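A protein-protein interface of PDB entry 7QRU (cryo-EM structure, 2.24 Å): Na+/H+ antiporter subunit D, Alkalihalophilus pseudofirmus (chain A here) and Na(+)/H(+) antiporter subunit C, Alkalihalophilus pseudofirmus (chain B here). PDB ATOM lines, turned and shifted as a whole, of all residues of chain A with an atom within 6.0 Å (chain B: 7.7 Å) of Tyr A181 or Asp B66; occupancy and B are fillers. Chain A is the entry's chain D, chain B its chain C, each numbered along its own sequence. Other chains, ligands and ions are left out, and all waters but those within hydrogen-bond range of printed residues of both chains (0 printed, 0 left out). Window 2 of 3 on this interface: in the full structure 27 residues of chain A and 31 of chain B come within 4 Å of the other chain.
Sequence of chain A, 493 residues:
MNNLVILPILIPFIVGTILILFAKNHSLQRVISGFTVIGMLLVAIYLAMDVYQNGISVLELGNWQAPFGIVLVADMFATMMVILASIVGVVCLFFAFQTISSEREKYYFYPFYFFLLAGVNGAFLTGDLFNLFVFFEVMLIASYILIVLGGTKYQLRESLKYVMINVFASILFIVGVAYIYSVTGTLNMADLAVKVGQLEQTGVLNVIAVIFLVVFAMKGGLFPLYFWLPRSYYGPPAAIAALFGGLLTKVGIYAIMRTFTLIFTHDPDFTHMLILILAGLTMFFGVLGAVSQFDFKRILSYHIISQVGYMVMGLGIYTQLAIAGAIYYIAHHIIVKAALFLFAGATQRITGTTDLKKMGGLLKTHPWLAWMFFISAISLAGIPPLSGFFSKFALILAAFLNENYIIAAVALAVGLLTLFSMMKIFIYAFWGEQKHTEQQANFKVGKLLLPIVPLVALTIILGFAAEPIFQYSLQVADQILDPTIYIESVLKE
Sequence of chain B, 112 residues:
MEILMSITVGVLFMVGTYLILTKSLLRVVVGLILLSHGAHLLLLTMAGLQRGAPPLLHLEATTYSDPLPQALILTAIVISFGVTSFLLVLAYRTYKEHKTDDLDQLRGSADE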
ATOM      1  N   GLY A 176     -19.475  12.334  10.748  1.00  0.00           N
ATOM      2  CA  GLY A 176     -18.861  11.377  11.646  1.00  0.00           C
ATOM      3  C   GLY A 176     -18.594  10.035  11.017  1.00  0.00           C
ATOM      4  O   GLY A 176     -17.619   9.386  11.346  1.00  0.00           O
ATOM      5  N   VAL A 177     -19.533   9.521  10.238  1.00  0.00           N
ATOM      6  CA  VAL A 177     -19.310   8.228   9.652  1.00  0.00           C
ATOM      7  C   VAL A 177     -18.200   8.345   8.622  1.00  0.00           C
ATOM      8  O   VAL A 177     -17.351   7.486   8.610  1.00  0.00           O
ATOM      9  CB  VAL A 177     -20.622   7.794   8.965  1.00  0.00           C
ATOM     10  CG1 VAL A 177     -20.394   6.738   7.909  1.00  0.00           C
ATOM     11  CG2 VAL A 177     -21.673   7.417   9.982  1.00  0.00           C
ATOM     12  N   ALA A 178     -18.134   9.444   7.858  1.00  0.00           N
ATOM     13  CA  ALA A 178     -17.003   9.629   6.954  1.00  0.00           C
ATOM     14  C   ALA A 178     -15.693   9.473   7.680  1.00  0.00           C
ATOM     15  O   ALA A 178     -14.858   8.688   7.260  1.00  0.00           O
ATOM     16  CB  ALA A 178     -17.093  10.950   6.313  1.00  0.00           C
ATOM     17  N   TYR A 179     -15.469  10.166   8.792  1.00  0.00           N
ATOM     18  CA  TYR A 179     -14.158  10.090   9.445  1.00  0.00           C
ATOM     19  C   TYR A 179     -13.847   8.728  10.084  1.00  0.00           C
ATOM     20  O   TYR A 179     -12.741   8.239   9.938  1.00  0.00           O
ATOM     21  CB  TYR A 179     -14.127  11.079  10.595  1.00  0.00           C
ATOM     22  CG  TYR A 179     -14.341  12.501  10.224  1.00  0.00           C
ATOM     23  CD1 TYR A 179     -13.697  13.052   9.125  1.00  0.00           C
ATOM     24  CD2 TYR A 179     -15.063  13.350  11.090  1.00  0.00           C
ATOM     25  CE1 TYR A 179     -13.805  14.401   8.867  1.00  0.00           C
ATOM     26  CE2 TYR A 179     -15.211  14.696  10.815  1.00  0.00           C
ATOM     27  CZ  TYR A 179     -14.560  15.226   9.694  1.00  0.00           C
ATOM     28  OH  TYR A 179     -14.605  16.560   9.454  1.00  0.00           O
ATOM     29  N   ILE A 180     -14.856   8.062  10.643  1.00  0.00           N
ATOM     30  CA  ILE A 180     -14.570   6.773  11.228  1.00  0.00           C
ATOM     31  C   ILE A 180     -14.354   5.715  10.141  1.00  0.00           C
ATOM     32  O   ILE A 180     -13.521   4.829  10.293  1.00  0.00           O
ATOM     33  CB  ILE A 180     -15.661   6.362  12.277  1.00  0.00           C
ATOM     34  CG1 ILE A 180     -15.041   5.560  13.419  1.00  0.00           C
ATOM     35  CG2 ILE A 180     -16.836   5.658  11.731  1.00  0.00           C
ATOM     36  CD1 ILE A 180     -16.121   5.297  14.408  1.00  0.00           C
ATOM     37  N   TYR A 181     -15.029   5.825   9.012  1.00  0.00           N
ATOM     38  CA  TYR A 181     -14.761   4.948   7.887  1.00  0.00           C
ATOM     39  C   TYR A 181     -13.323   5.118   7.384  1.00  0.00           C
ATOM     40  O   TYR A 181     -12.670   4.132   6.991  1.00  0.00           O
ATOM     41  CB  TYR A 181     -15.828   5.113   6.788  1.00  0.00           C
ATOM     42  CG  TYR A 181     -15.679   4.110   5.677  1.00  0.00           C
ATOM     43  CD1 TYR A 181     -16.186   2.825   5.833  1.00  0.00           C
ATOM     44  CD2 TYR A 181     -14.893   4.359   4.511  1.00  0.00           C
ATOM     45  CE1 TYR A 181     -15.991   1.874   4.834  1.00  0.00           C
ATOM     46  CE2 TYR A 181     -14.640   3.370   3.554  1.00  0.00           C
ATOM     47  CZ  TYR A 181     -15.288   2.158   3.671  1.00  0.00           C
ATOM     48  OH  TYR A 181     -15.072   1.188   2.787  1.00  0.00           O
ATOM     49  N   SER A 182     -12.849   6.335   7.292  1.00  0.00           N
ATOM     50  CA  SER A 182     -11.498   6.585   6.831  1.00  0.00           C
ATOM     51  C   SER A 182     -10.474   5.892   7.689  1.00  0.00           C
ATOM     52  O   SER A 182      -9.507   5.326   7.182  1.00  0.00           O
ATOM     53  CB  SER A 182     -11.211   8.079   6.827  1.00  0.00           C
ATOM     54  OG  SER A 182      -9.919   8.239   6.248  1.00  0.00           O
ATOM     55  N   VAL A 183     -10.733   5.871   9.012  1.00  0.00           N
ATOM     56  CA  VAL A 183      -9.804   5.280   9.960  1.00  0.00           C
ATOM     57  C   VAL A 183      -9.932   3.754   9.906  1.00  0.00           C
ATOM     58  O   VAL A 183      -8.952   3.027   9.998  1.00  0.00           O
ATOM     59  CB  VAL A 183     -10.052   5.828  11.392  1.00  0.00           C
ATOM     60  CG1 VAL A 183      -9.207   5.103  12.440  1.00  0.00           C
ATOM     61  CG2 VAL A 183      -9.854   7.328  11.417  1.00  0.00           C
ATOM     62  N   THR A 184     -11.121   3.218   9.816  1.00  0.00           N
ATOM     63  CA  THR A 184     -11.347   1.796  10.159  1.00  0.00           C
ATOM     64  C   THR A 184     -11.864   0.973   9.000  1.00  0.00           C
ATOM     65  O   THR A 184     -11.480  -0.185   8.969  1.00  0.00           O
ATOM     66  CB  THR A 184     -12.420   1.602  11.216  1.00  0.00           C
ATOM     67  OG1 THR A 184     -13.686   2.125  10.757  1.00  0.00           O
ATOM     68  CG2 THR A 184     -12.103   2.288  12.513  1.00  0.00           C
ATOM     69  N   GLY A 185     -12.552   1.578   8.012  1.00  0.00           N
ATOM     70  CA  GLY A 185     -12.972   0.784   6.904  1.00  0.00           C
ATOM     71  C   GLY A 185     -14.120  -0.161   7.245  1.00  0.00           C
ATOM     72  O   GLY A 185     -14.495  -0.992   6.429  1.00  0.00           O
ATOM     73  N   THR A 186     -14.853   0.108   8.327  1.00  0.00           N
ATOM     74  CA  THR A 186     -16.010  -0.691   8.670  1.00  0.00           C
ATOM     75  C   THR A 186     -17.130   0.193   9.202  1.00  0.00           C
ATOM     76  O   THR A 186     -16.867   1.243   9.760  1.00  0.00           O
ATOM     77  CB  THR A 186     -15.601  -1.800   9.678  1.00  0.00           C
ATOM     78  OG1 THR A 186     -16.750  -2.650   9.888  1.00  0.00           O
ATOM     79  CG2 THR A 186     -15.080  -1.266  11.004  1.00  0.00           C
ATOM     80  N   LEU A 187     -18.367  -0.308   9.116  1.00  0.00           N
ATOM     81  CA  LEU A 187     -19.523   0.303   9.711  1.00  0.00           C
ATOM     82  C   LEU A 187     -20.185  -0.531  10.800  1.00  0.00           C
ATOM     83  O   LEU A 187     -21.139  -0.078  11.432  1.00  0.00           O
ATOM     84  CB  LEU A 187     -20.484   0.530   8.549  1.00  0.00           C
ATOM     85  CG  LEU A 187     -19.926   1.442   7.432  1.00  0.00           C
ATOM     86  CD1 LEU A 187     -20.855   1.391   6.191  1.00  0.00           C
ATOM     87  CD2 LEU A 187     -19.653   2.869   7.954  1.00  0.00           C
ATOM     88  N   LEU B  43     -17.582  12.034   2.384  1.00  0.00           N
ATOM     89  CA  LEU B  43     -17.625  10.564   2.543  1.00  0.00           C
ATOM     90  C   LEU B  43     -16.894   9.892   1.405  1.00  0.00           C
ATOM     91  O   LEU B  43     -16.152   8.980   1.624  1.00  0.00           O
ATOM     92  CB  LEU B  43     -19.116  10.139   2.606  1.00  0.00           C
ATOM     93  CG  LEU B  43     -19.396   8.692   2.931  1.00  0.00           C
ATOM     94  CD1 LEU B  43     -18.496   8.130   3.944  1.00  0.00           C
ATOM     95  CD2 LEU B  43     -20.811   8.575   3.397  1.00  0.00           C
ATOM     96  N   LEU B  44     -16.960  10.447   0.184  1.00  0.00           N
ATOM     97  CA  LEU B  44     -16.150   9.913  -0.922  1.00  0.00           C
ATOM     98  C   LEU B  44     -14.678  10.140  -0.721  1.00  0.00           C
ATOM     99  O   LEU B  44     -13.875   9.244  -1.003  1.00  0.00           O
ATOM    100  CB  LEU B  44     -16.613  10.554  -2.233  1.00  0.00           C
ATOM    101  CG  LEU B  44     -16.220   9.805  -3.510  1.00  0.00           C
ATOM    102  CD1 LEU B  44     -16.881   8.453  -3.656  1.00  0.00           C
ATOM    103  CD2 LEU B  44     -16.610  10.653  -4.694  1.00  0.00           C
ATOM    104  N   MET B  46     -12.956  10.589   2.031  1.00  0.00           N
ATOM    105  CA  MET B  46     -12.431   9.835   3.143  1.00  0.00           C
ATOM    106  C   MET B  46     -12.140   8.407   2.750  1.00  0.00           C
ATOM    107  O   MET B  46     -11.207   7.800   3.295  1.00  0.00           O
ATOM    108  CB  MET B  46     -13.409   9.808   4.311  1.00  0.00           C
ATOM    109  CG  MET B  46     -13.499  11.092   5.127  1.00  0.00           C
ATOM    110  SD  MET B  46     -11.883  11.723   5.668  1.00  0.00           S
ATOM    111  CE  MET B  46     -11.457  12.870   4.384  1.00  0.00           C
ATOM    112  N   ALA B  47     -12.834   7.876   1.741  1.00  0.00           N
ATOM    113  CA  ALA B  47     -12.522   6.498   1.324  1.00  0.00           C
ATOM    114  C   ALA B  47     -11.243   6.340   0.506  1.00  0.00           C
ATOM    115  O   ALA B  47     -10.964   5.210   0.163  1.00  0.00           O
ATOM    116  CB  ALA B  47     -13.584   6.017   0.442  1.00  0.00           C
ATOM    117  N   GLY B  48     -10.621   7.454   0.044  1.00  0.00           N
ATOM    118  CA  GLY B  48      -9.439   7.523  -0.840  1.00  0.00           C
ATOM    119  C   GLY B  48      -9.913   7.843  -2.256  1.00  0.00           C
ATOM    120  O   GLY B  48     -10.960   7.379  -2.667  1.00  0.00           O
ATOM    121  N   GLN B  50      -9.405   8.112  -6.498  1.00  0.00           N
ATOM    122  CA  GLN B  50      -8.680   7.819  -7.722  1.00  0.00           C
ATOM    123  C   GLN B  50      -7.794   6.591  -7.535  1.00  0.00           C
ATOM    124  O   GLN B  50      -6.621   6.606  -7.923  1.00  0.00           O
ATOM    125  CB  GLN B  50      -7.816   9.003  -8.149  1.00  0.00           C
ATOM    126  CG  GLN B  50      -8.587  10.191  -8.579  1.00  0.00           C
ATOM    127  CD  GLN B  50      -7.662  11.342  -8.938  1.00  0.00           C
ATOM    128  OE1 GLN B  50      -7.911  11.957  -9.970  1.00  0.00           O
ATOM    129  NE2 GLN B  50      -6.667  11.677  -8.102  1.00  0.00           N
ATOM    130  N   ARG B  51      -8.338   5.629  -6.804  1.00  0.00           N
ATOM    131  CA  ARG B  51      -7.572   4.514  -6.303  1.00  0.00           C
ATOM    132  C   ARG B  51      -7.736   3.262  -7.162  1.00  0.00           C
ATOM    133  O   ARG B  51      -6.750   2.552  -7.264  1.00  0.00           O
ATOM    134  CB  ARG B  51      -7.976   4.183  -4.904  1.00  0.00           C
ATOM    135  CG  ARG B  51      -7.732   5.271  -3.875  1.00  0.00           C
ATOM    136  CD  ARG B  51      -6.347   5.617  -3.857  1.00  0.00           C
ATOM    137  NE  ARG B  51      -6.224   6.780  -2.990  1.00  0.00           N
ATOM    138  CZ  ARG B  51      -5.819   6.779  -1.736  1.00  0.00           C
ATOM    139  NH1 ARG B  51      -5.742   5.645  -1.072  1.00  0.00           N
ATOM    140  NH2 ARG B  51      -5.624   7.929  -1.114  1.00  0.00           N
ATOM    141  N   GLY B  52      -8.752   3.219  -7.998  1.00  0.00           N
ATOM    142  CA  GLY B  52      -8.795   2.364  -9.145  1.00  0.00           C
ATOM    143  C   GLY B  52     -10.017   2.628 -10.031  1.00  0.00           C
ATOM    144  O   GLY B  52     -10.567   3.741 -10.055  1.00  0.00           O
ATOM    145  N   ALA B  53     -10.434   1.584 -10.749  1.00  0.00           N
ATOM    146  CA  ALA B  53     -11.425   1.750 -11.752  1.00  0.00           C
ATOM    147  C   ALA B  53     -12.756   2.027 -11.086  1.00  0.00           C
ATOM    148  O   ALA B  53     -13.017   1.581  -9.960  1.00  0.00           O
ATOM    149  CB  ALA B  53     -11.440   0.460 -12.498  1.00  0.00           C
ATOM    150  N   PRO B  54     -13.737   2.492 -11.850  1.00  0.00           N
ATOM    151  CA  PRO B  54     -15.095   2.513 -11.352  1.00  0.00           C
ATOM    152  C   PRO B  54     -15.475   1.075 -10.956  1.00  0.00           C
ATOM    153  O   PRO B  54     -15.005   0.062 -11.480  1.00  0.00           O
ATOM    154  CB  PRO B  54     -15.923   3.055 -12.524  1.00  0.00           C
ATOM    155  CG  PRO B  54     -14.876   3.498 -13.486  1.00  0.00           C
ATOM    156  CD  PRO B  54     -13.618   2.708 -13.259  1.00  0.00           C
ATOM    157  N   PRO B  55     -16.300   0.898  -9.931  1.00  0.00           N
ATOM    158  CA  PRO B  55     -16.465  -0.452  -9.363  1.00  0.00           C
ATOM    159  C   PRO B  55     -17.428  -1.357 -10.150  1.00  0.00           C
ATOM    160  O   PRO B  55     -18.456  -1.800  -9.631  1.00  0.00           O
ATOM    161  CB  PRO B  55     -16.932  -0.124  -7.943  1.00  0.00           C
ATOM    162  CG  PRO B  55     -17.532   1.259  -8.028  1.00  0.00           C
ATOM    163  CD  PRO B  55     -16.972   1.989  -9.226  1.00  0.00           C
ATOM    164  N   THR B  63      -7.483  -2.876  -9.346  1.00  0.00           N
ATOM    165  CA  THR B  63      -7.900  -2.154  -8.173  1.00  0.00           C
ATOM    166  C   THR B  63      -9.193  -1.493  -8.558  1.00  0.00           C
ATOM    167  O   THR B  63      -9.325  -1.068  -9.664  1.00  0.00           O
ATOM    168  CB  THR B  63      -6.778  -1.200  -7.718  1.00  0.00           C
ATOM    169  OG1 THR B  63      -5.754  -1.906  -7.032  1.00  0.00           O
ATOM    170  CG2 THR B  63      -7.214  -0.311  -6.609  1.00  0.00           C
ATOM    171  N   TYR B  64     -10.166  -1.492  -7.693  1.00  0.00           N
ATOM    172  CA  TYR B  64     -11.343  -0.734  -7.988  1.00  0.00           C
ATOM    173  C   TYR B  64     -11.414   0.353  -6.969  1.00  0.00           C
ATOM    174  O   TYR B  64     -10.904   0.130  -5.914  1.00  0.00           O
ATOM    175  CB  TYR B  64     -12.577  -1.579  -7.802  1.00  0.00           C
ATOM    176  CG  TYR B  64     -12.624  -2.651  -8.813  1.00  0.00           C
ATOM    177  CD1 TYR B  64     -13.156  -2.336 -10.049  1.00  0.00           C
ATOM    178  CD2 TYR B  64     -12.054  -3.907  -8.560  1.00  0.00           C
ATOM    179  CE1 TYR B  64     -13.169  -3.287 -11.050  1.00  0.00           C
ATOM    180  CE2 TYR B  64     -12.022  -4.824  -9.577  1.00  0.00           C
ATOM    181  CZ  TYR B  64     -12.576  -4.507 -10.826  1.00  0.00           C
ATOM    182  OH  TYR B  64     -12.637  -5.346 -11.901  1.00  0.00           O
ATOM    183  N   SER B  65     -12.026   1.494  -7.303  1.00  0.00           N
ATOM    184  CA  SER B  65     -12.351   2.481  -6.290  1.00  0.00           C
ATOM    185  C   SER B  65     -13.307   1.807  -5.280  1.00  0.00           C
ATOM    186  O   SER B  65     -14.092   0.984  -5.636  1.00  0.00           O
ATOM    187  CB  SER B  65     -12.996   3.610  -6.937  1.00  0.00           C
ATOM    188  OG  SER B  65     -14.232   3.070  -7.461  1.00  0.00           O
ATOM    189  N   ASP B  66     -13.308   2.199  -4.022  1.00  0.00           N
ATOM    190  CA  ASP B  66     -14.038   1.510  -2.992  1.00  0.00           C
ATOM    191  C   ASP B  66     -15.549   1.632  -3.222  1.00  0.00           C
ATOM    192  O   ASP B  66     -16.068   2.727  -3.314  1.00  0.00           O
ATOM    193  CB  ASP B  66     -13.670   2.147  -1.653  1.00  0.00           C
ATOM    194  CG  ASP B  66     -14.211   1.434  -0.430  1.00  0.00           C
ATOM    195  OD1 ASP B  66     -15.069   0.442  -0.575  1.00  0.00           O
ATOM    196  OD2 ASP B  66     -13.822   1.885   0.631  1.00  0.00           O
ATOM    197  N   PRO B  67     -16.312   0.519  -3.379  1.00  0.00           N
ATOM    198  CA  PRO B  67     -17.717   0.621  -3.699  1.00  0.00           C
ATOM    199  C   PRO B  67     -18.557   0.861  -2.455  1.00  0.00           C
ATOM    200  O   PRO B  67     -19.630   1.448  -2.585  1.00  0.00           O
ATOM    201  CB  PRO B  67     -18.049  -0.717  -4.247  1.00  0.00           C
ATOM    202  CG  PRO B  67     -17.160  -1.603  -3.384  1.00  0.00           C
ATOM    203  CD  PRO B  67     -15.833  -0.852  -3.393  1.00  0.00           C
ATOM    204  N   LEU B  68     -18.068   0.564  -1.248  1.00  0.00           N
ATOM    205  CA  LEU B  68     -19.001   0.716  -0.148  1.00  0.00           C
ATOM    206  C   LEU B  68     -19.395   2.161   0.096  1.00  0.00           C
ATOM    207  O   LEU B  68     -20.579   2.521   0.207  1.00  0.00           O
ATOM    208  CB  LEU B  68     -18.441   0.087   1.100  1.00  0.00           C
ATOM    209  CG  LEU B  68     -19.331   0.207   2.336  1.00  0.00           C
ATOM    210  CD1 LEU B  68     -20.717  -0.268   2.132  1.00  0.00           C
ATOM    211  CD2 LEU B  68     -18.657  -0.609   3.407  1.00  0.00           C
ATOM    212  N   PRO B  69     -18.491   3.134   0.066  1.00  0.00           N
ATOM    213  CA  PRO B  69     -18.909   4.528   0.242  1.00  0.00           C
ATOM    214  C   PRO B  69     -19.825   5.043  -0.835  1.00  0.00           C
ATOM    215  O   PRO B  69     -20.584   5.929  -0.603  1.00  0.00           O
ATOM    216  CB  PRO B  69     -17.607   5.281   0.125  1.00  0.00           C
ATOM    217  CG  PRO B  69     -16.605   4.323   0.371  1.00  0.00           C
ATOM    218  CD  PRO B  69     -17.077   2.970  -0.066  1.00  0.00           C
ATOM    219  N   GLN B  70     -19.613   4.588  -2.062  1.00  0.00           N
ATOM    220  CA  GLN B  70     -20.464   4.964  -3.137  1.00  0.00           C
ATOM    221  C   GLN B  70     -21.850   4.509  -2.803  1.00  0.00           C
ATOM    222  O   GLN B  70     -22.795   5.285  -2.986  1.00  0.00           O
ATOM    223  CB  GLN B  70     -19.934   4.368  -4.445  1.00  0.00           C
ATOM    224  CG  GLN B  70     -18.551   4.904  -4.843  1.00  0.00           C
ATOM    225  CD  GLN B  70     -18.160   4.607  -6.275  1.00  0.00           C
ATOM    226  OE1 GLN B  70     -19.061   4.455  -7.094  1.00  0.00           O
ATOM    227  NE2 GLN B  70     -16.860   4.639  -6.639  1.00  0.00           N
ATOM    228  N   ALA B  71     -22.038   3.288  -2.240  1.00  0.00           N
ATOM    229  CA  ALA B  71     -23.435   2.899  -1.909  1.00  0.00           C
ATOM    230  C   ALA B  71     -23.951   3.701  -0.732  1.00  0.00           C
ATOM    231  O   ALA B  71     -25.099   4.142  -0.787  1.00  0.00           O
ATOM    232  CB  ALA B  71     -23.408   1.486  -1.545  1.00  0.00           C
ATOM    233  N   LEU B  72     -23.075   4.062   0.251  1.00  0.00           N
ATOM    234  CA  LEU B  72     -23.567   4.915   1.331  1.00  0.00           C
ATOM    235  C   LEU B  72     -24.012   6.261   0.798  1.00  0.00           C
ATOM    236  O   LEU B  72     -25.105   6.720   1.148  1.00  0.00           O
ATOM    237  CB  LEU B  72     -22.552   5.153   2.426  1.00  0.00           C
ATOM    238  CG  LEU B  72     -21.941   3.884   3.064  1.00  0.00           C
ATOM    239  CD1 LEU B  72     -21.202   4.286   4.306  1.00  0.00           C
ATOM    240  CD2 LEU B  72     -22.936   2.810   3.403  1.00  0.00           C
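OH of Tyr A181 sits at hydrogen-bond distance from OD2 of Asp B66, 2.6 Å away.
The side-chain hydroxyl (OG) of Ser A182 lies within hydrogen-bond range of the backbone carbonyl oxygen (O) of Met B46 (3.3 Å).
OD1 of Asp B66 lies within hydrogen-bond range of N of Leu B68 (3.1 Å).
Among the printed residues, pairs that only touch across the chains: Ala A178 with Met B46 (3.5 Å), Leu A187 with Leu B72 (3.5 Å), Ala A178 with Leu B43 (3.7 Å), Tyr A181 with Pro B69 (3.9 Å) and Tyr A181 with Leu B68 (3.9 Å).
Printed residues of chain B within 4 Å of Ser A182: Met B46.
Gly A185 touches none of the printed residues of chain B.
Of the printed residues of chain B, Leu A187 touches Leu B72.
Printed residues of chain A within 4 Å of Asp B66: Tyr A181 (2.6 Å).
Pro B67 touches none of the printed residues of chain A.
Printed residues of chain A within 4 Å of Pro B69: Tyr A181.
Of the printed residues of chain A, Leu B72 touches Leu A187.
The nearest residue of chain B that does not touch Tyr A181 is Ala B47 (4.2 Å).
The nearest printed residue of chain A that does not touch Asp B66 is Gly A185 (6.4 Å).
Hydrophobic or aromatic side chains of chain B within 4 Å of the printed part of chain A: Leu B43, Met B46, Leu B68, Pro B69 and Leu B72.
Among the printed residues, no Asp or Glu carboxylate lies within 4 Å of a Lys or Arg side-chain nitrogen of the other chain.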
